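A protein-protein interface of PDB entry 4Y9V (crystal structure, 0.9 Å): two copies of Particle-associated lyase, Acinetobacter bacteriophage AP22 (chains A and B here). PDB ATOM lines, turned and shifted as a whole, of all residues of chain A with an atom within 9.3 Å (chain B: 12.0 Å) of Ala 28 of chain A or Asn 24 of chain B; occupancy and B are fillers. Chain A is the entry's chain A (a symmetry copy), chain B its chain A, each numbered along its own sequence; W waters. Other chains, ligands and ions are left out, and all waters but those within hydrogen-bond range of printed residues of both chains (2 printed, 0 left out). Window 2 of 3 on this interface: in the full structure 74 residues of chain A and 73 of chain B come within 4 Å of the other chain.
Water W1 lies within hydrogen-bond range of the side-chain hydroxyl of Ser 25 of chain B (2.7 Å), the side-chain amide oxygen of Gln 38 of chain B (2.7 Å), the backbone NH of Ser 27 of chain B (3.1 Å), the backbone NH of Ala 26 of chain B (3.3 Å) and the backbone carbonyl oxygen of Leu 30 of chain A (3.4 Å). Water W2 bridges the backbone carbonyl oxygen (O) of Leu 30 of chain A and the side-chain hydroxyl (OG) of Ser 25 of chain B.
Among the printed residues, pairs that only touch across the chains: Ile 29 of chain A with Asn 24 of chain B, Ile 29 of chain A with Ser 25 of chain B, Ile 29 of chain A with Ala 26 of chain B, Leu 30 of chain A with Ser 25 of chain B, Gln 37 of chain A with Ala 26 of chain B and Gln 37 of chain A with Gln 37 of chain B.
Ala 28 of chain A touches Asn 24 of chain B, but with the chains exchanged Asn 24 of chain A does not touch Ala 28 of chain B (9.7 Å). Ile 29 of chain A touches Asn 24 of chain B, but with the chains exchanged Asn 24 of chain A does not touch Ile 29 of chain B (6.7 Å). Ile 29 of chain A touches Ala 26 of chain B, but with the chains exchanged Ala 26 of chain A does not touch Ile 29 of chain B (8.2 Å). Leu 30 of chain A touches Ser 25 of chain B, but with the chains exchanged Ser 25 of chain A does not touch Leu 30 of chain B (12.1 Å). Of the 13 pairs that touch across the chains among the printed residues, 1 has its exchanged pair printed and touching as well.
N of Gln 37 of chain B is in hydrogen-bond range of O of Ile 29 of chain B (2.8 Å). The backbone NH (N) of Gln 37 of chain A sits at hydrogen-bond distance from the backbone carbonyl oxygen (O) of Ile 29 of chain A, at 2.8 Å. The side-chain amide oxygen (OD1) of Asn 41 of chain B sits at hydrogen-bond distance from the side-chain amide nitrogen (NE2) of Gln 37 of chain B (3.1 Å). O of Ala 26 of chain B sits at hydrogen-bond distance from N of Gln 37 of chain B. The backbone carbonyl oxygen of Ala 26 of chain B sits at hydrogen-bond distance from the backbone NH of Gln 38 of chain B. The side-chain hydroxyl of Ser 36 of chain B sits close to the backbone NH of Gln 38 of chain B.
Printed residues of chain B that touch a printed residue of chain A: Asn 24, Ser 25, Ala 26, Gln 37, Gln 38 and Asn 41. Hydrophobic or aromatic side chains of chain B that line the printed part of chain A: Ala 26. Hydrophobic or aromatic side chains of chain A that line the printed part of chain B: Ala 28, Ile 29 and Leu 30. Along chain A the printed residues that touch a printed residue of chain B span positions 28 to 37. Among the printed residues, 13 pairs touch across the chains.
Ala 28 of chain A touches just one residue of chain B: Asn 24 (2.9 Å). No residue of chain B comes within 4 Å of Ala 23 of chain A. No residue of chain B comes within 4 Å of Asn 24 of chain A. No residue of chain A comes within 4 Å of Ala 23 of chain B. Of the printed residues of chain A, Asn 41 of chain B touches Asp 31 and Gln 37. Printed residues of chain B within 4 Å of Gln 37 of chain A: Ala 26, Gln 37 and Asn 41. Ile 35 of chain A touches none of the printed residues of chain B. The nearest printed residue of chain B that does not touch Ala 28 of chain A is Ser 25 of chain B (5.6 Å). The nearest printed residue of chain A that does not touch Asn 24 of chain B is Ala 23 of chain A (4.1 Å). The nearest printed residue of chain B that does not touch Leu 30 of chain A is Gln 38 of chain B (4.4 Å).
The side-chain amide oxygen of Asn 24 of chain B sits close to the backbone carbonyl oxygen of Ala 28 of chain A (2.9 Å). N of Ala 26 of chain B sits at hydrogen-bond distance from O of Leu 30 of chain A (2.9 Å). N of Lys 32 of chain A sits at hydrogen-bond distance from OE1 of Gln 38 of chain B (2.9 Å). The side-chain amide oxygen of Gln 37 of chain A is in hydrogen-bond range of the side-chain amide nitrogen of Asn 41 of chain B (2.8 Å). ND2 of Asn 41 of chain B lies within hydrogen-bond range of OD1 of Asp 31 of chain A (3.0 Å). NE2 of Gln 38 of chain B is in hydrogen-bond range of OD1 of Asp 31 of chain A, at 3.0 Å. The backbone carbonyl oxygen of Asn 24 of chain B sits at hydrogen-bond distance from the backbone NH of Leu 30 of chain A, at 2.8 Å.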
ATOM      1  N   ALA A  23      -0.517   7.378  -3.841  1.00  0.00           N
ATOM      2  CA  ALA A  23       0.162   8.303  -2.914  1.00  0.00           C
ATOM      3  C   ALA A  23      -0.848   8.832  -1.902  1.00  0.00           C
ATOM      4  O   ALA A  23      -0.548   9.524  -0.926  1.00  0.00           O
ATOM      5  CB  ALA A  23       0.829   9.453  -3.647  1.00  0.00           C
ATOM      6  N   ASN A  24      -2.119   8.449  -2.195  1.00  0.00           N
ATOM      7  CA  ASN A  24      -3.179   8.991  -1.428  1.00  0.00           C
ATOM      8  C   ASN A  24      -3.665   8.017  -0.356  1.00  0.00           C
ATOM      9  O   ASN A  24      -4.719   8.285   0.226  1.00  0.00           O
ATOM     10  CB  ASN A  24      -4.411   9.457  -2.225  1.00  0.00           C
ATOM     11  CG  ASN A  24      -3.986  10.857  -2.703  1.00  0.00           C
ATOM     12  OD1 ASN A  24      -4.248  11.873  -2.041  1.00  0.00           O
ATOM     13  ND2 ASN A  24      -3.277  10.809  -3.825  1.00  0.00           N
ATOM     14  N   SER A  25      -2.920   7.006  -0.049  1.00  0.00           N
ATOM     15  CA  SER A  25      -3.229   6.073   1.018  1.00  0.00           C
ATOM     16  C   SER A  25      -2.794   6.618   2.367  1.00  0.00           C
ATOM     17  O   SER A  25      -1.761   7.273   2.449  1.00  0.00           O
ATOM     18  CB  SER A  25      -2.434   4.824   0.668  1.00  0.00           C
ATOM     19  OG  SER A  25      -2.571   3.898   1.740  1.00  0.00           O
ATOM     20  N   ALA A  26      -3.514   6.278   3.417  1.00  0.00           N
ATOM     21  CA  ALA A  26      -3.069   6.602   4.774  1.00  0.00           C
ATOM     22  C   ALA A  26      -1.718   5.954   5.075  1.00  0.00           C
ATOM     23  O   ALA A  26      -0.931   6.479   5.873  1.00  0.00           O
ATOM     24  CB  ALA A  26      -4.102   6.199   5.807  1.00  0.00           C
ATOM     25  N   SER A  27      -1.380   4.859   4.406  1.00  0.00           N
ATOM     26  CA  SER A  27      -0.102   4.251   4.559  1.00  0.00           C
ATOM     27  C   SER A  27       1.050   5.109   4.046  1.00  0.00           C
ATOM     28  O   SER A  27       2.213   4.843   4.410  1.00  0.00           O
ATOM     29  CB  SER A  27      -0.068   2.942   3.766  1.00  0.00           C
ATOM     30  OG  SER A  27      -0.779   2.015   4.548  1.00  0.00           O
ATOM     31  N   ALA A  28       0.764   6.106   3.200  1.00  0.00           N
ATOM     32  CA  ALA A  28       1.784   6.995   2.617  1.00  0.00           C
ATOM     33  C   ALA A  28       2.061   8.219   3.463  1.00  0.00           C
ATOM     34  O   ALA A  28       2.969   8.962   3.110  1.00  0.00           O
ATOM     35  CB  ALA A  28       1.335   7.368   1.200  1.00  0.00           C
ATOM     36  N   ILE A  29       1.289   8.434   4.491  1.00  0.00           N
ATOM     37  CA  ILE A  29       1.384   9.632   5.346  1.00  0.00           C
ATOM     38  C   ILE A  29       2.125   9.252   6.608  1.00  0.00           C
ATOM     39  O   ILE A  29       1.804   8.218   7.199  1.00  0.00           O
ATOM     40  CB  ILE A  29      -0.005  10.181   5.632  1.00  0.00           C
ATOM     41  CG1 ILE A  29      -0.767  10.518   4.334  1.00  0.00           C
ATOM     42  CG2 ILE A  29       0.052  11.356   6.568  1.00  0.00           C
ATOM     43  CD1 ILE A  29      -0.064  11.445   3.360  1.00  0.00           C
ATOM     44  N   LEU A  30       3.104  10.078   6.996  1.00  0.00           N
ATOM     45  CA  LEU A  30       3.968   9.754   8.121  1.00  0.00           C
ATOM     46  C   LEU A  30       3.630  10.601   9.350  1.00  0.00           C
ATOM     47  O   LEU A  30       3.682  11.814   9.268  1.00  0.00           O
ATOM     48  CB  LEU A  30       5.400   9.995   7.614  1.00  0.00           C
ATOM     49  CG  LEU A  30       6.533   9.525   8.501  1.00  0.00           C
ATOM     50  CD1 LEU A  30       6.396   8.041   8.816  1.00  0.00           C
ATOM     51  CD2 LEU A  30       7.867   9.834   7.811  1.00  0.00           C
ATOM     52  N   ASP A  31       3.262   9.943  10.458  1.00  0.00           N
ATOM     53  CA  ASP A  31       3.149  10.622  11.726  1.00  0.00           C
ATOM     54  C   ASP A  31       4.549  11.014  12.208  1.00  0.00           C
ATOM     55  O   ASP A  31       5.517  10.336  11.864  1.00  0.00           O
ATOM     56  CB  ASP A  31       2.448   9.687  12.716  1.00  0.00           C
ATOM     57  CG  ASP A  31       2.249  10.300  14.101  1.00  0.00           C
ATOM     58  OD1 ASP A  31       1.288  11.057  14.287  1.00  0.00           O
ATOM     59  OD2 ASP A  31       3.091   9.953  15.013  1.00  0.00           O
ATOM     60  N   LYS A  32       4.648  12.042  13.041  1.00  0.00           N
ATOM     61  CA  LYS A  32       5.939  12.474  13.562  1.00  0.00           C
ATOM     62  C   LYS A  32       6.672  11.370  14.310  1.00  0.00           C
ATOM     63  O   LYS A  32       7.907  11.420  14.434  1.00  0.00           O
ATOM     64  CB  LYS A  32       5.804  13.700  14.444  1.00  0.00           C
ATOM     65  CG  LYS A  32       5.181  13.511  15.769  1.00  0.00           C
ATOM     66  CD  LYS A  32       5.209  14.778  16.679  1.00  0.00           C
ATOM     67  CE  LYS A  32       4.326  14.477  17.930  1.00  0.00           C
ATOM     68  NZ  LYS A  32       4.241  15.625  18.854  1.00  0.00           N
ATOM     69  N   ILE A  35       5.563   6.099  12.685  1.00  0.00           N
ATOM     70  CA  ILE A  35       4.542   5.187  12.166  1.00  0.00           C
ATOM     71  C   ILE A  35       3.710   5.906  11.129  1.00  0.00           C
ATOM     72  O   ILE A  35       3.597   7.141  11.116  1.00  0.00           O
ATOM     73  CB  ILE A  35       3.685   4.542  13.274  1.00  0.00           C
ATOM     74  CG1 ILE A  35       2.611   5.438  13.871  1.00  0.00           C
ATOM     75  CG2 ILE A  35       4.581   3.929  14.361  1.00  0.00           C
ATOM     76  CD1 ILE A  35       1.716   4.741  14.896  1.00  0.00           C
ATOM     77  N   SER A  36       3.055   5.154  10.219  1.00  0.00           N
ATOM     78  CA  SER A  36       2.217   5.758   9.220  1.00  0.00           C
ATOM     79  C   SER A  36       0.876   6.174   9.811  1.00  0.00           C
ATOM     80  O   SER A  36       0.457   5.714  10.863  1.00  0.00           O
ATOM     81  CB  SER A  36       1.956   4.819   8.047  1.00  0.00           C
ATOM     82  OG  SER A  36       0.995   3.839   8.396  1.00  0.00           O
ATOM     83  N   GLN A  37       0.147   7.007   9.041  1.00  0.00           N
ATOM     84  CA  GLN A  37      -1.203   7.369   9.477  1.00  0.00           C
ATOM     85  C   GLN A  37      -2.093   6.137   9.520  1.00  0.00           C
ATOM     86  O   GLN A  37      -2.988   6.065  10.381  1.00  0.00           O
ATOM     87  CB  GLN A  37      -1.785   8.436   8.534  1.00  0.00           C
ATOM     88  CG  GLN A  37      -3.133   8.918   8.999  1.00  0.00           C
ATOM     89  CD  GLN A  37      -2.991   9.650  10.324  1.00  0.00           C
ATOM     90  OE1 GLN A  37      -2.116  10.516  10.471  1.00  0.00           O
ATOM     91  NE2 GLN A  37      -3.859   9.343  11.297  1.00  0.00           N
ATOM     92  N   GLN A  38      -1.911   5.183   8.627  1.00  0.00           N
ATOM     93  CA  GLN A  38      -2.686   3.931   8.730  1.00  0.00           C
ATOM     94  C   GLN A  38      -2.434   3.252  10.062  1.00  0.00           C
ATOM     95  O   GLN A  38      -3.361   2.749  10.703  1.00  0.00           O
ATOM     96  CB  GLN A  38      -2.410   2.974   7.587  1.00  0.00           C
ATOM     97  CG  GLN A  38      -3.321   1.763   7.594  1.00  0.00           C
ATOM     98  CD  GLN A  38      -4.760   2.158   7.415  1.00  0.00           C
ATOM     99  OE1 GLN A  38      -5.139   2.712   6.366  1.00  0.00           O
ATOM    100  NE2 GLN A  38      -5.592   1.903   8.421  1.00  0.00           N
ATOM    101  N   GLU A  39      -1.170   3.197  10.469  1.00  0.00           N
ATOM    102  CA  GLU A  39      -0.824   2.574  11.761  1.00  0.00           C
ATOM    103  C   GLU A  39      -1.421   3.345  12.925  1.00  0.00           C
ATOM    104  O   GLU A  39      -1.869   2.752  13.904  1.00  0.00           O
ATOM    105  CB  GLU A  39       0.689   2.458  11.895  1.00  0.00           C
ATOM    106  CG  GLU A  39       1.312   1.510  10.893  1.00  0.00           C
ATOM    107  CD  GLU A  39       2.796   1.456  11.088  1.00  0.00           C
ATOM    108  OE1 GLU A  39       3.294   0.541  11.794  1.00  0.00           O
ATOM    109  OE2 GLU A  39       3.507   2.350  10.584  1.00  0.00           O
ATOM    110  N   ALA B  23       6.003  16.099   1.550  1.00  0.00           N
ATOM    111  CA  ALA B  23       4.567  16.356   1.336  1.00  0.00           C
ATOM    112  C   ALA B  23       3.753  15.236   1.973  1.00  0.00           C
ATOM    113  O   ALA B  23       2.523  15.243   2.066  1.00  0.00           O
ATOM    114  CB  ALA B  23       4.227  16.484  -0.139  1.00  0.00           C
ATOM    115  N   ASN B  24       4.540  14.226   2.432  1.00  0.00           N
ATOM    116  CA  ASN B  24       3.914  13.051   2.912  1.00  0.00           C
ATOM    117  C   ASN B  24       3.846  13.022   4.438  1.00  0.00           C
ATOM    118  O   ASN B  24       3.525  11.960   4.977  1.00  0.00           O
ATOM    119  CB  ASN B  24       4.542  11.722   2.451  1.00  0.00           C
ATOM    120  CG  ASN B  24       3.921  11.532   1.054  1.00  0.00           C
ATOM    121  OD1 ASN B  24       2.873  10.889   0.895  1.00  0.00           O
ATOM    122  ND2 ASN B  24       4.599  12.180   0.114  1.00  0.00           N
ATOM    123  N   SER B  25       4.045  14.119   5.091  1.00  0.00           N
ATOM    124  CA  SER B  25       3.910  14.235   6.532  1.00  0.00           C
ATOM    125  C   SER B  25       2.458  14.433   6.931  1.00  0.00           C
ATOM    126  O   SER B  25       1.723  15.110   6.223  1.00  0.00           O
ATOM    127  CB  SER B  25       4.731  15.463   6.889  1.00  0.00           C
ATOM    128  OG  SER B  25       4.542  15.734   8.274  1.00  0.00           O
ATOM    129  N   ALA B  26       2.077  13.931   8.089  1.00  0.00           N
ATOM    130  CA  ALA B  26       0.753  14.227   8.641  1.00  0.00           C
ATOM    131  C   ALA B  26       0.575  15.730   8.856  1.00  0.00           C
ATOM    132  O   ALA B  26      -0.548  16.247   8.790  1.00  0.00           O
ATOM    133  CB  ALA B  26       0.505  13.465   9.926  1.00  0.00           C
ATOM    134  N   SER B  27       1.658  16.474   9.039  1.00  0.00           N
ATOM    135  CA  SER B  27       1.585  17.891   9.152  1.00  0.00           C
ATOM    136  C   SER B  27       1.135  18.585   7.870  1.00  0.00           C
ATOM    137  O   SER B  27       0.725  19.760   7.929  1.00  0.00           O
ATOM    138  CB  SER B  27       2.972  18.443   9.492  1.00  0.00           C
ATOM    139  OG  SER B  27       3.149  18.183  10.861  1.00  0.00           O
ATOM    140  N   ALA B  28       1.223  17.903   6.722  1.00  0.00           N
ATOM    141  CA  ALA B  28       0.841  18.463   5.413  1.00  0.00           C
ATOM    142  C   ALA B  28      -0.614  18.230   5.068  1.00  0.00           C
ATOM    143  O   ALA B  28      -1.048  18.750   4.047  1.00  0.00           O
ATOM    144  CB  ALA B  28       1.780  17.877   4.353  1.00  0.00           C
ATOM    145  N   ILE B  29      -1.308  17.454   5.853  1.00  0.00           N
ATOM    146  CA  ILE B  29      -2.706  17.067   5.589  1.00  0.00           C
ATOM    147  C   ILE B  29      -3.603  17.919   6.458  1.00  0.00           C
ATOM    148  O   ILE B  29      -3.320  18.057   7.651  1.00  0.00           O
ATOM    149  CB  ILE B  29      -2.893  15.579   5.846  1.00  0.00           C
ATOM    150  CG1 ILE B  29      -1.937  14.725   4.987  1.00  0.00           C
ATOM    151  CG2 ILE B  29      -4.327  15.168   5.663  1.00  0.00           C
ATOM    152  CD1 ILE B  29      -1.970  14.972   3.490  1.00  0.00           C
ATOM    153  N   LEU B  30      -4.656  18.483   5.855  1.00  0.00           N
ATOM    154  CA  LEU B  30      -5.519  19.421   6.556  1.00  0.00           C
ATOM    155  C   LEU B  30      -6.864  18.789   6.915  1.00  0.00           C
ATOM    156  O   LEU B  30      -7.565  18.339   6.026  1.00  0.00           O
ATOM    157  CB  LEU B  30      -5.666  20.622   5.607  1.00  0.00           C
ATOM    158  CG  LEU B  30      -6.331  21.863   6.163  1.00  0.00           C
ATOM    159  CD1 LEU B  30      -5.615  22.348   7.416  1.00  0.00           C
ATOM    160  CD2 LEU B  30      -6.359  22.944   5.075  1.00  0.00           C
ATOM    161  N   SER B  36      -4.002  20.499  11.346  1.00  0.00           N
ATOM    162  CA  SER B  36      -3.413  19.470  10.532  1.00  0.00           C
ATOM    163  C   SER B  36      -3.757  18.086  11.067  1.00  0.00           C
ATOM    164  O   SER B  36      -4.144  17.908  12.213  1.00  0.00           O
ATOM    165  CB  SER B  36      -1.895  19.595  10.460  1.00  0.00           C
ATOM    166  OG  SER B  36      -1.297  19.123  11.655  1.00  0.00           O
ATOM    167  N   GLN B  37      -3.507  17.068  10.219  1.00  0.00           N
ATOM    168  CA  GLN B  37      -3.702  15.696  10.689  1.00  0.00           C
ATOM    169  C   GLN B  37      -2.740  15.386  11.826  1.00  0.00           C
ATOM    170  O   GLN B  37      -3.101  14.612  12.731  1.00  0.00           O
ATOM    171  CB  GLN B  37      -3.506  14.713   9.520  1.00  0.00           C
ATOM    172  CG  GLN B  37      -3.795  13.294   9.929  1.00  0.00           C
ATOM    173  CD  GLN B  37      -5.268  13.147  10.280  1.00  0.00           C
ATOM    174  OE1 GLN B  37      -6.139  13.595   9.521  1.00  0.00           O
ATOM    175  NE2 GLN B  37      -5.574  12.496  11.410  1.00  0.00           N
ATOM    176  N   GLN B  38      -1.537  15.926  11.814  1.00  0.00           N
ATOM    177  CA  GLN B  38      -0.639  15.731  12.968  1.00  0.00           C
ATOM    178  C   GLN B  38      -1.274  16.260  14.239  1.00  0.00           C
ATOM    179  O   GLN B  38      -1.198  15.629  15.297  1.00  0.00           O
ATOM    180  CB  GLN B  38       0.728  16.354  12.762  1.00  0.00           C
ATOM    181  CG  GLN B  38       1.708  16.017  13.866  1.00  0.00           C
ATOM    182  CD  GLN B  38       1.974  14.539  13.931  1.00  0.00           C
ATOM    183  OE1 GLN B  38       2.511  13.950  12.975  1.00  0.00           O
ATOM    184  NE2 GLN B  38       1.602  13.899  15.037  1.00  0.00           N
ATOM    185  N   GLU B  39      -1.874  17.443  14.154  1.00  0.00           N
ATOM    186  CA  GLU B  39      -2.540  18.033  15.329  1.00  0.00           C
ATOM    187  C   GLU B  39      -3.724  17.194  15.777  1.00  0.00           C
ATOM    188  O   GLU B  39      -3.967  17.043  16.971  1.00  0.00           O
ATOM    189  CB  GLU B  39      -2.964  19.465  15.024  1.00  0.00           C
ATOM    190  CG  GLU B  39      -1.799  20.404  14.797  1.00  0.00           C
ATOM    191  CD  GLU B  39      -2.299  21.784  14.500  1.00  0.00           C
ATOM    192  OE1 GLU B  39      -2.390  22.623  15.433  1.00  0.00           O
ATOM    193  OE2 GLU B  39      -2.662  22.060  13.338  1.00  0.00           O
ATOM    194  N   ASN B  41      -3.892  13.909  15.428  1.00  0.00           N
ATOM    195  CA  ASN B  41      -3.213  12.769  16.055  1.00  0.00           C
ATOM    196  C   ASN B  41      -2.721  13.121  17.457  1.00  0.00           C
ATOM    197  O   ASN B  41      -2.793  12.288  18.360  1.00  0.00           O
ATOM    198  CB  ASN B  41      -2.047  12.296  15.200  1.00  0.00           C
ATOM    199  CG  ASN B  41      -2.415  11.729  13.830  1.00  0.00           C
ATOM    200  OD1 ASN B  41      -3.577  11.522  13.514  1.00  0.00           O
ATOM    201  ND2 ASN B  41      -1.381  11.469  13.045  1.00  0.00           N
HETATM  202  O   HOH W   1       3.766  14.895  10.729  1.00  0.00           O
HETATM  203  O   HOH W   2       5.920  13.497   9.749  1.00  0.00           O
